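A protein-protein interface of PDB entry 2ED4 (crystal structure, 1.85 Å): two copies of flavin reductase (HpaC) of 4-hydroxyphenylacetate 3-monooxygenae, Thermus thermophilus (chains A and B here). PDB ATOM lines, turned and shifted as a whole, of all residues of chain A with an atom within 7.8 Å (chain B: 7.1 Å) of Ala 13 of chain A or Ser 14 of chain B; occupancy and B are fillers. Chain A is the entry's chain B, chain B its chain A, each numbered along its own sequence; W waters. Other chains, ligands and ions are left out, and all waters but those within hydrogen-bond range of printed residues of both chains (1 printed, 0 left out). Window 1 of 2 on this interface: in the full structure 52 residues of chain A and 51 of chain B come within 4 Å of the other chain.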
ATOM      1  N   ALA A   8     -30.593 -20.897  29.211  1.00  0.00           N
ATOM      2  CA  ALA A   8     -30.898 -22.148  28.528  1.00  0.00           C
ATOM      3  C   ALA A   8     -29.727 -22.588  27.646  1.00  0.00           C
ATOM      4  O   ALA A   8     -29.285 -23.737  27.721  1.00  0.00           O
ATOM      5  CB  ALA A   8     -32.163 -21.990  27.686  1.00  0.00           C
ATOM      6  N   LEU A   9     -29.219 -21.681  26.820  1.00  0.00           N
ATOM      7  CA  LEU A   9     -28.100 -22.026  25.949  1.00  0.00           C
ATOM      8  C   LEU A   9     -26.810 -22.263  26.730  1.00  0.00           C
ATOM      9  O   LEU A   9     -25.940 -23.004  26.278  1.00  0.00           O
ATOM     10  CB  LEU A   9     -27.896 -20.951  24.874  1.00  0.00           C
ATOM     11  CG  LEU A   9     -28.722 -21.097  23.585  1.00  0.00           C
ATOM     12  CD1 LEU A   9     -28.409 -22.438  22.916  1.00  0.00           C
ATOM     13  CD2 LEU A   9     -30.209 -21.004  23.894  1.00  0.00           C
ATOM     14  N   ALA A  10     -26.682 -21.646  27.904  1.00  0.00           N
ATOM     15  CA  ALA A  10     -25.489 -21.853  28.728  1.00  0.00           C
ATOM     16  C   ALA A  10     -25.510 -23.302  29.204  1.00  0.00           C
ATOM     17  O   ALA A  10     -24.496 -23.845  29.638  1.00  0.00           O
ATOM     18  CB  ALA A  10     -25.492 -20.908  29.935  1.00  0.00           C
ATOM     19  N   ARG A  11     -26.680 -23.926  29.116  1.00  0.00           N
ATOM     20  CA  ARG A  11     -26.827 -25.305  29.537  1.00  0.00           C
ATOM     21  C   ARG A  11     -26.577 -26.307  28.421  1.00  0.00           C
ATOM     22  O   ARG A  11     -26.790 -27.503  28.600  1.00  0.00           O
ATOM     23  CB  ARG A  11     -28.203 -25.523  30.165  1.00  0.00           C
ATOM     24  CG  ARG A  11     -28.353 -24.757  31.465  1.00  0.00           C
ATOM     25  CD  ARG A  11     -29.721 -24.933  32.092  1.00  0.00           C
ATOM     26  NE  ARG A  11     -29.843 -24.104  33.286  1.00  0.00           N
ATOM     27  CZ  ARG A  11     -30.804 -24.230  34.196  1.00  0.00           C
ATOM     28  NH1 ARG A  11     -31.741 -25.158  34.056  1.00  0.00           N
ATOM     29  NH2 ARG A  11     -30.823 -23.429  35.252  1.00  0.00           N
ATOM     30  N   PHE A  12     -26.138 -25.819  27.263  1.00  0.00           N
ATOM     31  CA  PHE A  12     -25.801 -26.722  26.173  1.00  0.00           C
ATOM     32  C   PHE A  12     -24.283 -26.734  26.119  1.00  0.00           C
ATOM     33  O   PHE A  12     -23.658 -25.744  25.723  1.00  0.00           O
ATOM     34  CB  PHE A  12     -26.337 -26.255  24.818  1.00  0.00           C
ATOM     35  CG  PHE A  12     -26.019 -27.212  23.698  1.00  0.00           C
ATOM     36  CD1 PHE A  12     -26.617 -28.470  23.655  1.00  0.00           C
ATOM     37  CD2 PHE A  12     -25.078 -26.886  22.727  1.00  0.00           C
ATOM     38  CE1 PHE A  12     -26.280 -29.391  22.663  1.00  0.00           C
ATOM     39  CE2 PHE A  12     -24.734 -27.802  21.731  1.00  0.00           C
ATOM     40  CZ  PHE A  12     -25.335 -29.057  21.700  1.00  0.00           C
ATOM     41  N   ALA A  13     -23.697 -27.851  26.529  1.00  0.00           N
ATOM     42  CA  ALA A  13     -22.252 -27.998  26.535  1.00  0.00           C
ATOM     43  C   ALA A  13     -21.743 -28.189  25.118  1.00  0.00           C
ATOM     44  O   ALA A  13     -22.463 -28.686  24.251  1.00  0.00           O
ATOM     45  CB  ALA A  13     -21.857 -29.201  27.397  1.00  0.00           C
ATOM     46  N   SER A  14     -20.500 -27.790  24.877  1.00  0.00           N
ATOM     47  CA  SER A  14     -19.918 -27.964  23.556  1.00  0.00           C
ATOM     48  C   SER A  14     -18.408 -27.848  23.584  1.00  0.00           C
ATOM     49  O   SER A  14     -17.824 -27.336  24.542  1.00  0.00           O
ATOM     50  CB  SER A  14     -20.466 -26.916  22.589  1.00  0.00           C
ATOM     51  OG  SER A  14     -19.921 -25.647  22.878  1.00  0.00           O
ATOM     52  N   GLY A  15     -17.781 -28.342  22.523  1.00  0.00           N
ATOM     53  CA  GLY A  15     -16.347 -28.226  22.404  1.00  0.00           C
ATOM     54  C   GLY A  15     -16.133 -26.782  21.998  1.00  0.00           C
ATOM     55  O   GLY A  15     -17.103 -26.027  21.857  1.00  0.00           O
ATOM     56  N   THR A  33     -18.131 -21.523  19.575  1.00  0.00           N
ATOM     57  CA  THR A  33     -18.681 -22.758  20.113  1.00  0.00           C
ATOM     58  C   THR A  33     -19.884 -23.140  19.248  1.00  0.00           C
ATOM     59  O   THR A  33     -20.336 -24.280  19.280  1.00  0.00           O
ATOM     60  CB  THR A  33     -19.142 -22.617  21.574  1.00  0.00           C
ATOM     61  OG1 THR A  33     -19.916 -21.419  21.722  1.00  0.00           O
ATOM     62  CG2 THR A  33     -17.942 -22.598  22.509  1.00  0.00           C
ATOM     63  N   PHE A  35     -20.830 -24.460  16.482  1.00  0.00           N
ATOM     64  CA  PHE A  35     -20.306 -25.313  15.422  1.00  0.00           C
ATOM     65  C   PHE A  35     -21.033 -26.642  15.496  1.00  0.00           C
ATOM     66  O   PHE A  35     -21.401 -27.091  16.578  1.00  0.00           O
ATOM     67  CB  PHE A  35     -18.809 -25.561  15.652  1.00  0.00           C
ATOM     68  CG  PHE A  35     -18.220 -26.631  14.771  1.00  0.00           C
ATOM     69  CD1 PHE A  35     -17.843 -26.351  13.462  1.00  0.00           C
ATOM     70  CD2 PHE A  35     -18.049 -27.926  15.255  1.00  0.00           C
ATOM     71  CE1 PHE A  35     -17.301 -27.347  12.645  1.00  0.00           C
ATOM     72  CE2 PHE A  35     -17.509 -28.929  14.447  1.00  0.00           C
ATOM     73  CZ  PHE A  35     -17.133 -28.638  13.140  1.00  0.00           C
ATOM     74  N   MET A  36     -21.237 -27.274  14.348  1.00  0.00           N
ATOM     75  CA  MET A  36     -21.905 -28.565  14.328  1.00  0.00           C
ATOM     76  C   MET A  36     -21.678 -29.291  13.019  1.00  0.00           C
ATOM     77  O   MET A  36     -21.465 -28.669  11.973  1.00  0.00           O
ATOM     78  CB  MET A  36     -23.414 -28.405  14.558  1.00  0.00           C
ATOM     79  CG  MET A  36     -24.139 -27.537  13.529  1.00  0.00           C
ATOM     80  SD  MET A  36     -25.924 -27.452  13.847  1.00  0.00           S
ATOM     81  CE  MET A  36     -26.505 -26.747  12.293  1.00  0.00           C
ATOM     82  N   PRO A 134     -11.054 -33.084  25.162  1.00  0.00           N
ATOM     83  CA  PRO A 134     -11.261 -31.770  24.553  1.00  0.00           C
ATOM     84  C   PRO A 134     -11.450 -30.608  25.517  1.00  0.00           C
ATOM     85  O   PRO A 134     -11.596 -30.799  26.725  1.00  0.00           O
ATOM     86  CB  PRO A 134     -12.520 -32.001  23.740  1.00  0.00           C
ATOM     87  CG  PRO A 134     -13.347 -32.789  24.740  1.00  0.00           C
ATOM     88  CD  PRO A 134     -12.342 -33.788  25.326  1.00  0.00           C
ATOM     89  N   VAL A 136     -13.887 -27.959  26.762  1.00  0.00           N
ATOM     90  CA  VAL A 136     -15.341 -27.899  26.778  1.00  0.00           C
ATOM     91  C   VAL A 136     -15.808 -26.597  27.414  1.00  0.00           C
ATOM     92  O   VAL A 136     -15.134 -26.051  28.288  1.00  0.00           O
ATOM     93  CB  VAL A 136     -15.922 -29.090  27.591  1.00  0.00           C
ATOM     94  CG1 VAL A 136     -17.445 -29.020  27.625  1.00  0.00           C
ATOM     95  CG2 VAL A 136     -15.467 -30.411  26.976  1.00  0.00           C
ATOM     96  N   TYR A 137     -16.953 -26.092  26.963  1.00  0.00           N
ATOM     97  CA  TYR A 137     -17.513 -24.874  27.529  1.00  0.00           C
ATOM     98  C   TYR A 137     -18.941 -25.218  27.935  1.00  0.00           C
ATOM     99  O   TYR A 137     -19.689 -25.807  27.159  1.00  0.00           O
ATOM    100  CB  TYR A 137     -17.514 -23.730  26.506  1.00  0.00           C
ATOM    101  CG  TYR A 137     -17.570 -22.360  27.152  1.00  0.00           C
ATOM    102  CD1 TYR A 137     -16.454 -21.826  27.796  1.00  0.00           C
ATOM    103  CD2 TYR A 137     -18.749 -21.615  27.153  1.00  0.00           C
ATOM    104  CE1 TYR A 137     -16.508 -20.581  28.428  1.00  0.00           C
ATOM    105  CE2 TYR A 137     -18.819 -20.371  27.783  1.00  0.00           C
ATOM    106  CZ  TYR A 137     -17.695 -19.861  28.419  1.00  0.00           C
ATOM    107  OH  TYR A 137     -17.766 -18.642  29.057  1.00  0.00           O
ATOM    108  N   PHE A 138     -19.303 -24.866  29.161  1.00  0.00           N
ATOM    109  CA  PHE A 138     -20.628 -25.157  29.692  1.00  0.00           C
ATOM    110  C   PHE A 138     -20.845 -24.273  30.904  1.00  0.00           C
ATOM    111  O   PHE A 138     -19.947 -24.129  31.735  1.00  0.00           O
ATOM    112  CB  PHE A 138     -20.706 -26.627  30.120  1.00  0.00           C
ATOM    113  CG  PHE A 138     -21.974 -26.993  30.852  1.00  0.00           C
ATOM    114  CD1 PHE A 138     -23.188 -27.091  30.174  1.00  0.00           C
ATOM    115  CD2 PHE A 138     -21.949 -27.262  32.218  1.00  0.00           C
ATOM    116  CE1 PHE A 138     -24.356 -27.455  30.845  1.00  0.00           C
ATOM    117  CE2 PHE A 138     -23.110 -27.627  32.900  1.00  0.00           C
ATOM    118  CZ  PHE A 138     -24.317 -27.725  32.213  1.00  0.00           C
ATOM    119  N   GLN A 139     -22.035 -23.694  31.003  1.00  0.00           N
ATOM    120  CA  GLN A 139     -22.377 -22.829  32.126  1.00  0.00           C
ATOM    121  C   GLN A 139     -21.371 -21.719  32.381  1.00  0.00           C
ATOM    122  O   GLN A 139     -20.896 -21.531  33.499  1.00  0.00           O
ATOM    123  CB  GLN A 139     -22.578 -23.666  33.397  1.00  0.00           C
ATOM    124  CG  GLN A 139     -23.967 -24.270  33.498  1.00  0.00           C
ATOM    125  CD  GLN A 139     -25.048 -23.223  33.718  1.00  0.00           C
ATOM    126  OE1 GLN A 139     -24.814 -22.022  33.567  1.00  0.00           O
ATOM    127  NE2 GLN A 139     -26.242 -23.679  34.068  1.00  0.00           N
ATOM    128  N   ARG A 143     -14.645 -26.337  30.954  1.00  0.00           N
ATOM    129  CA  ARG A 143     -14.796 -27.533  31.766  1.00  0.00           C
ATOM    130  C   ARG A 143     -13.967 -28.669  31.197  1.00  0.00           C
ATOM    131  O   ARG A 143     -13.449 -28.578  30.085  1.00  0.00           O
ATOM    132  CB  ARG A 143     -16.266 -27.959  31.783  1.00  0.00           C
ATOM    133  CG  ARG A 143     -17.253 -26.827  32.020  1.00  0.00           C
ATOM    134  CD  ARG A 143     -17.158 -26.269  33.428  1.00  0.00           C
ATOM    135  NE  ARG A 143     -18.038 -25.116  33.597  1.00  0.00           N
ATOM    136  CZ  ARG A 143     -18.167 -24.431  34.728  1.00  0.00           C
ATOM    137  NH1 ARG A 143     -17.470 -24.783  35.802  1.00  0.00           N
ATOM    138  NH2 ARG A 143     -18.993 -23.394  34.786  1.00  0.00           N
ATOM    139  N   LEU A 145     -13.759 -33.116  30.769  1.00  0.00           N
ATOM    140  CA  LEU A 145     -14.549 -34.340  30.771  1.00  0.00           C
ATOM    141  C   LEU A 145     -13.906 -35.330  31.734  1.00  0.00           C
ATOM    142  O   LEU A 145     -12.688 -35.315  31.925  1.00  0.00           O
ATOM    143  CB  LEU A 145     -14.559 -34.987  29.385  1.00  0.00           C
ATOM    144  CG  LEU A 145     -15.229 -34.279  28.210  1.00  0.00           C
ATOM    145  CD1 LEU A 145     -15.134 -35.163  26.971  1.00  0.00           C
ATOM    146  CD2 LEU A 145     -16.687 -34.000  28.549  1.00  0.00           C
ATOM    147  N   PHE B  12     -15.526 -33.460  18.480  1.00  0.00           N
ATOM    148  CA  PHE B  12     -16.197 -32.236  18.884  1.00  0.00           C
ATOM    149  C   PHE B  12     -17.241 -32.650  19.900  1.00  0.00           C
ATOM    150  O   PHE B  12     -18.255 -33.260  19.542  1.00  0.00           O
ATOM    151  CB  PHE B  12     -16.905 -31.534  17.724  1.00  0.00           C
ATOM    152  CG  PHE B  12     -17.536 -30.230  18.127  1.00  0.00           C
ATOM    153  CD1 PHE B  12     -16.741 -29.125  18.418  1.00  0.00           C
ATOM    154  CD2 PHE B  12     -18.914 -30.115  18.266  1.00  0.00           C
ATOM    155  CE1 PHE B  12     -17.306 -27.924  18.843  1.00  0.00           C
ATOM    156  CE2 PHE B  12     -19.494 -28.917  18.692  1.00  0.00           C
ATOM    157  CZ  PHE B  12     -18.689 -27.820  18.980  1.00  0.00           C
ATOM    158  N   ALA B  13     -16.988 -32.337  21.166  1.00  0.00           N
ATOM    159  CA  ALA B  13     -17.917 -32.686  22.231  1.00  0.00           C
ATOM    160  C   ALA B  13     -19.165 -31.822  22.121  1.00  0.00           C
ATOM    161  O   ALA B  13     -19.116 -30.718  21.579  1.00  0.00           O
ATOM    162  CB  ALA B  13     -17.262 -32.473  23.585  1.00  0.00           C
ATOM    163  N   SER B  14     -20.283 -32.328  22.625  1.00  0.00           N
ATOM    164  CA  SER B  14     -21.523 -31.565  22.589  1.00  0.00           C
ATOM    165  C   SER B  14     -22.557 -32.133  23.538  1.00  0.00           C
ATOM    166  O   SER B  14     -22.497 -33.307  23.920  1.00  0.00           O
ATOM    167  CB  SER B  14     -22.115 -31.576  21.184  1.00  0.00           C
ATOM    168  OG  SER B  14     -22.628 -32.859  20.886  1.00  0.00           O
ATOM    169  N   GLY B  15     -23.506 -31.290  23.918  1.00  0.00           N
ATOM    170  CA  GLY B  15     -24.581 -31.750  24.770  1.00  0.00           C
ATOM    171  C   GLY B  15     -25.436 -32.600  23.851  1.00  0.00           C
ATOM    172  O   GLY B  15     -25.134 -32.725  22.655  1.00  0.00           O
ATOM    173  N   VAL B  16     -26.498 -33.184  24.384  1.00  0.00           N
ATOM    174  CA  VAL B  16     -27.379 -34.012  23.573  1.00  0.00           C
ATOM    175  C   VAL B  16     -28.787 -33.452  23.701  1.00  0.00           C
ATOM    176  O   VAL B  16     -29.240 -33.157  24.805  1.00  0.00           O
ATOM    177  CB  VAL B  16     -27.355 -35.475  24.056  1.00  0.00           C
ATOM    178  CG1 VAL B  16     -28.245 -36.340  23.170  1.00  0.00           C
ATOM    179  CG2 VAL B  16     -25.919 -35.998  24.040  1.00  0.00           C
ATOM    180  N   THR B  17     -29.469 -33.288  22.572  1.00  0.00           N
ATOM    181  CA  THR B  17     -30.826 -32.756  22.587  1.00  0.00           C
ATOM    182  C   THR B  17     -31.823 -33.725  21.972  1.00  0.00           C
ATOM    183  O   THR B  17     -31.453 -34.703  21.318  1.00  0.00           O
ATOM    184  CB  THR B  17     -30.949 -31.437  21.783  1.00  0.00           C
ATOM    185  OG1 THR B  17     -31.031 -31.735  20.381  1.00  0.00           O
ATOM    186  CG2 THR B  17     -29.743 -30.538  22.033  1.00  0.00           C
ATOM    187  N   ALA B  32     -30.630 -35.399  18.766  1.00  0.00           N
ATOM    188  CA  ALA B  32     -29.730 -34.632  17.916  1.00  0.00           C
ATOM    189  C   ALA B  32     -28.631 -33.935  18.701  1.00  0.00           C
ATOM    190  O   ALA B  32     -28.890 -33.348  19.750  1.00  0.00           O
ATOM    191  CB  ALA B  32     -30.524 -33.593  17.117  1.00  0.00           C
ATOM    192  N   THR B  33     -27.402 -34.016  18.191  1.00  0.00           N
ATOM    193  CA  THR B  33     -26.265 -33.346  18.815  1.00  0.00           C
ATOM    194  C   THR B  33     -25.940 -32.115  17.974  1.00  0.00           C
ATOM    195  O   THR B  33     -25.296 -31.177  18.450  1.00  0.00           O
ATOM    196  CB  THR B  33     -25.013 -34.247  18.881  1.00  0.00           C
ATOM    197  OG1 THR B  33     -24.794 -34.858  17.603  1.00  0.00           O
ATOM    198  CG2 THR B  33     -25.175 -35.320  19.960  1.00  0.00           C
ATOM    199  N   ALA B  34     -26.392 -32.118  16.723  1.00  0.00           N
ATOM    200  CA  ALA B  34     -26.155 -30.990  15.826  1.00  0.00           C
ATOM    201  C   ALA B  34     -27.124 -29.869  16.181  1.00  0.00           C
ATOM    202  O   ALA B  34     -28.179 -29.703  15.560  1.00  0.00           O
ATOM    203  CB  ALA B  34     -26.336 -31.413  14.370  1.00  0.00           C
ATOM    204  N   PHE B  35     -26.743 -29.103  17.196  1.00  0.00           N
ATOM    205  CA  PHE B  35     -27.540 -27.995  17.706  1.00  0.00           C
ATOM    206  C   PHE B  35     -26.594 -26.878  18.129  1.00  0.00           C
ATOM    207  O   PHE B  35     -25.476 -27.141  18.570  1.00  0.00           O
ATOM    208  CB  PHE B  35     -28.350 -28.467  18.926  1.00  0.00           C
ATOM    209  CG  PHE B  35     -28.990 -27.350  19.713  1.00  0.00           C
ATOM    210  CD1 PHE B  35     -30.214 -26.811  19.323  1.00  0.00           C
ATOM    211  CD2 PHE B  35     -28.363 -26.838  20.853  1.00  0.00           C
ATOM    212  CE1 PHE B  35     -30.813 -25.775  20.059  1.00  0.00           C
ATOM    213  CE2 PHE B  35     -28.949 -25.802  21.598  1.00  0.00           C
ATOM    214  CZ  PHE B  35     -30.178 -25.268  21.201  1.00  0.00           C
ATOM    215  N   LEU B  69     -32.731 -30.051  26.251  1.00  0.00           N
ATOM    216  CA  LEU B  69     -31.317 -30.298  26.522  1.00  0.00           C
ATOM    217  C   LEU B  69     -31.228 -31.340  27.627  1.00  0.00           C
ATOM    218  O   LEU B  69     -31.612 -31.080  28.768  1.00  0.00           O
ATOM    219  CB  LEU B  69     -30.627 -29.007  26.961  1.00  0.00           C
ATOM    220  CG  LEU B  69     -30.857 -27.784  26.066  1.00  0.00           C
ATOM    221  CD1 LEU B  69     -29.991 -26.636  26.551  1.00  0.00           C
ATOM    222  CD2 LEU B  69     -30.527 -28.118  24.620  1.00  0.00           C
ATOM    223  N   LEU B 100     -32.464 -30.285  31.307  1.00  0.00           N
ATOM    224  CA  LEU B 100     -31.814 -29.083  31.821  1.00  0.00           C
ATOM    225  C   LEU B 100     -32.573 -27.842  31.373  1.00  0.00           C
ATOM    226  O   LEU B 100     -32.680 -26.861  32.111  1.00  0.00           O
ATOM    227  CB  LEU B 100     -30.371 -29.004  31.327  1.00  0.00           C
ATOM    228  CG  LEU B 100     -29.329 -29.631  32.251  1.00  0.00           C
ATOM    229  CD1 LEU B 100     -28.015 -29.816  31.505  1.00  0.00           C
ATOM    230  CD2 LEU B 100     -29.143 -28.728  33.472  1.00  0.00           C
ATOM    231  N   PRO B 134     -24.563 -31.862  32.488  1.00  0.00           N
ATOM    232  CA  PRO B 134     -25.257 -32.241  31.258  1.00  0.00           C
ATOM    233  C   PRO B 134     -24.872 -33.619  30.738  1.00  0.00           C
ATOM    234  O   PRO B 134     -23.901 -34.226  31.193  1.00  0.00           O
ATOM    235  CB  PRO B 134     -24.810 -31.160  30.288  1.00  0.00           C
ATOM    236  CG  PRO B 134     -23.337 -31.054  30.647  1.00  0.00           C
ATOM    237  CD  PRO B 134     -23.358 -31.065  32.180  1.00  0.00           C
ATOM    238  N   LEU B 135     -25.657 -34.105  29.784  1.00  0.00           N
ATOM    239  CA  LEU B 135     -25.366 -35.368  29.129  1.00  0.00           C
ATOM    240  C   LEU B 135     -24.472 -34.910  27.985  1.00  0.00           C
ATOM    241  O   LEU B 135     -24.855 -34.028  27.214  1.00  0.00           O
ATOM    242  CB  LEU B 135     -26.634 -36.000  28.555  1.00  0.00           C
ATOM    243  CG  LEU B 135     -26.398 -37.304  27.786  1.00  0.00           C
ATOM    244  CD1 LEU B 135     -25.838 -38.353  28.736  1.00  0.00           C
ATOM    245  CD2 LEU B 135     -27.703 -37.787  27.163  1.00  0.00           C
ATOM    246  N   VAL B 136     -23.277 -35.479  27.889  1.00  0.00           N
ATOM    247  CA  VAL B 136     -22.348 -35.093  26.836  1.00  0.00           C
ATOM    248  C   VAL B 136     -22.013 -36.281  25.949  1.00  0.00           C
ATOM    249  O   VAL B 136     -21.968 -37.424  26.416  1.00  0.00           O
ATOM    250  CB  VAL B 136     -21.021 -34.547  27.426  1.00  0.00           C
ATOM    251  CG1 VAL B 136     -20.060 -34.167  26.300  1.00  0.00           C
ATOM    252  CG2 VAL B 136     -21.297 -33.343  28.309  1.00  0.00           C
ATOM    253  N   TYR B 137     -21.793 -36.004  24.669  1.00  0.00           N
ATOM    254  CA  TYR B 137     -21.418 -37.036  23.722  1.00  0.00           C
ATOM    255  C   TYR B 137     -20.066 -36.627  23.151  1.00  0.00           C
ATOM    256  O   TYR B 137     -19.872 -35.478  22.745  1.00  0.00           O
ATOM    257  CB  TYR B 137     -22.437 -37.154  22.591  1.00  0.00           C
ATOM    258  CG  TYR B 137     -22.394 -38.508  21.917  1.00  0.00           C
ATOM    259  CD1 TYR B 137     -22.848 -39.648  22.581  1.00  0.00           C
ATOM    260  CD2 TYR B 137     -21.873 -38.657  20.633  1.00  0.00           C
ATOM    261  CE1 TYR B 137     -22.786 -40.907  21.980  1.00  0.00           C
ATOM    262  CE2 TYR B 137     -21.807 -39.909  20.021  1.00  0.00           C
ATOM    263  CZ  TYR B 137     -22.265 -41.029  20.701  1.00  0.00           C
ATOM    264  OH  TYR B 137     -22.197 -42.268  20.100  1.00  0.00           O
ATOM    265  N   PHE B 138     -19.131 -37.565  23.134  1.00  0.00           N
ATOM    266  CA  PHE B 138     -17.790 -37.298  22.626  1.00  0.00           C
ATOM    267  C   PHE B 138     -17.113 -38.633  22.345  1.00  0.00           C
ATOM    268  O   PHE B 138     -17.230 -39.571  23.137  1.00  0.00           O
ATOM    269  CB  PHE B 138     -16.992 -36.514  23.673  1.00  0.00           C
ATOM    270  CG  PHE B 138     -15.541 -36.314  23.322  1.00  0.00           C
ATOM    271  CD1 PHE B 138     -15.160 -35.401  22.340  1.00  0.00           C
ATOM    272  CD2 PHE B 138     -14.551 -37.029  23.990  1.00  0.00           C
ATOM    273  CE1 PHE B 138     -13.816 -35.202  22.031  1.00  0.00           C
ATOM    274  CE2 PHE B 138     -13.208 -36.842  23.691  1.00  0.00           C
ATOM    275  CZ  PHE B 138     -12.838 -35.923  22.706  1.00  0.00           C
ATOM    276  N   LEU B 145     -19.028 -34.606  32.725  1.00  0.00           N
ATOM    277  CA  LEU B 145     -18.134 -33.487  32.957  1.00  0.00           C
ATOM    278  C   LEU B 145     -17.604 -33.559  34.380  1.00  0.00           C
ATOM    279  O   LEU B 145     -18.263 -34.109  35.264  1.00  0.00           O
ATOM    280  CB  LEU B 145     -18.880 -32.162  32.820  1.00  0.00           C
ATOM    281  CG  LEU B 145     -19.392 -31.687  31.466  1.00  0.00           C
ATOM    282  CD1 LEU B 145     -20.004 -30.299  31.647  1.00  0.00           C
ATOM    283  CD2 LEU B 145     -18.245 -31.638  30.470  1.00  0.00           C
HETATM  284  O   HOH W   1     -22.822 -27.619  18.695  1.00  0.00           O
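Ala 13 of chain A touches just these residues of chain B: Ser 14 and Gly 15.
Of chain A, only Ala 13 (3.5 Å) comes within 4 Å of Ser 14 of chain B.
Of chain A, only Ser 14 and Gly 15 come within 4 Å of Ala 13 of chain B.
Of the printed residues of chain B, Phe 12 of chain A touches Gly 15, Thr 17, Thr 33 and Phe 35.
Of the printed residues of chain A, Phe 35 of chain B touches Leu 9 (3.7 Å), Phe 12 (3.3 Å) and Met 36 (3.8 Å).
Printed residues of chain B within 4 Å of Phe 138 of chain A: Pro 134 (3.5 Å) and Leu 145 (3.7 Å).
Printed residues of chain B within 4 Å of Arg 11 of chain A: Leu 69 and Leu 100.
Of the printed residues of chain A, Thr 17 of chain B touches Phe 12.
The nearest residue of chain A that does not touch Ser 14 of chain B is Ser 14 of chain A (4.1 Å).
The nearest printed residue of chain B that does not touch Ala 8 of chain A is Leu 100 of chain B (6.2 Å).
The guanidinium group (NE) of Arg 143 of chain A is in hydrogen-bond range of the backbone carbonyl oxygen (O) of Phe 138 of chain A (2.8 Å).
OG1 of Thr 17 of chain B is in hydrogen-bond range of O of Ala 32 of chain B, at 2.8 Å.
The backbone carbonyl oxygen (O) of Val 136 of chain A is in hydrogen-bond range of the backbone NH (N) of Arg 143 of chain A (2.7 Å).
The backbone NH of Tyr 137 of chain B lies within hydrogen-bond range of the backbone carbonyl oxygen of Ser 14 of chain B, 2.9 Å away.
N of Leu 100 of chain B lies within hydrogen-bond range of O of Leu 69 of chain B (2.8 Å).
N of Tyr 137 of chain A is in hydrogen-bond range of O of Ser 14 of chain A (2.9 Å).
Among the printed residues, pairs that only touch across the chains: Ala 8 of chain A with Leu 69 of chain B (3.2 Å), Phe 12 of chain A with Phe 35 of chain B (3.3 Å), Phe 35 of chain A with Phe 12 of chain B (3.4 Å), Pro 134 of chain A with Phe 138 of chain B (3.4 Å), Leu 145 of chain A with Leu 145 of chain B (3.4 Å), Ala 13 of chain A with Ser 14 of chain B (3.5 Å), Phe 138 of chain A with Pro 134 of chain B (3.5 Å), Ser 14 of chain A with Ala 13 of chain B (3.5 Å), Phe 12 of chain A with Gly 15 of chain B (3.5 Å), Gly 15 of chain A with Phe 12 of chain B (3.6 Å), Leu 145 of chain A with Phe 138 of chain B (3.6 Å), Phe 138 of chain A with Leu 145 of chain B (3.7 Å), Leu 9 of chain A with Phe 35 of chain B (3.7 Å), Phe 12 of chain A with Thr 17 of chain B (3.7 Å), Met 36 of chain A with Phe 35 of chain B (3.8 Å), Phe 12 of chain A with Thr 33 of chain B (3.9 Å), Arg 11 of chain A with Leu 69 of chain B (3.9 Å), Thr 33 of chain A with Phe 12 of chain B (3.9 Å) and Val 136 of chain A with Leu 145 of chain B (3.9 Å).
Water W1 lies within hydrogen-bond range of O of Phe 35 of chain A (2.6 Å) and O of Phe 35 of chain B (2.7 Å).
Phe 12 of chain A touches Thr 33 of chain B, and with the chains exchanged Thr 33 of chain A touches Phe 12 of chain B.
Ala 13 of chain A touches Ser 14 of chain B, and with the chains exchanged Ser 14 of chain A touches Ala 13 of chain B.
Val 136 of chain A touches Leu 145 of chain B, but with the chains exchanged Leu 145 of chain A does not touch Val 136 of chain B (4.1 Å).
Phe 138 of chain A touches Leu 145 of chain B, and with the chains exchanged Leu 145 of chain A touches Phe 138 of chain B.
11 positions are printed for both chains.
Of the 23 pairs that touch across the chains among the printed residues, 15 have their exchanged pair printed and touching as well.
The backbone carbonyl oxygen of Ala 13 of chain B lies within hydrogen-bond range of the backbone NH of Gly 15 of chain A, 2.9 Å away.
The backbone NH (N) of Gly 15 of chain B lies within hydrogen-bond range of the backbone carbonyl oxygen (O) of Ala 13 of chain A, 2.8 Å away.
The guanidinium group (NH1) of Arg 11 of chain A lies within hydrogen-bond range of the backbone carbonyl oxygen (O) of Leu 100 of chain B (2.8 Å).
O of Ala 34 of chain B sits close to SD of Met 36 of chain A, 3.6 Å away.
Of the 18 printed residues of chain B, 13 touch a printed residue of chain A.
Among the printed residues, no Asp or Glu carboxylate lies within 4 Å of a Lys or Arg side-chain nitrogen of the other chain.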
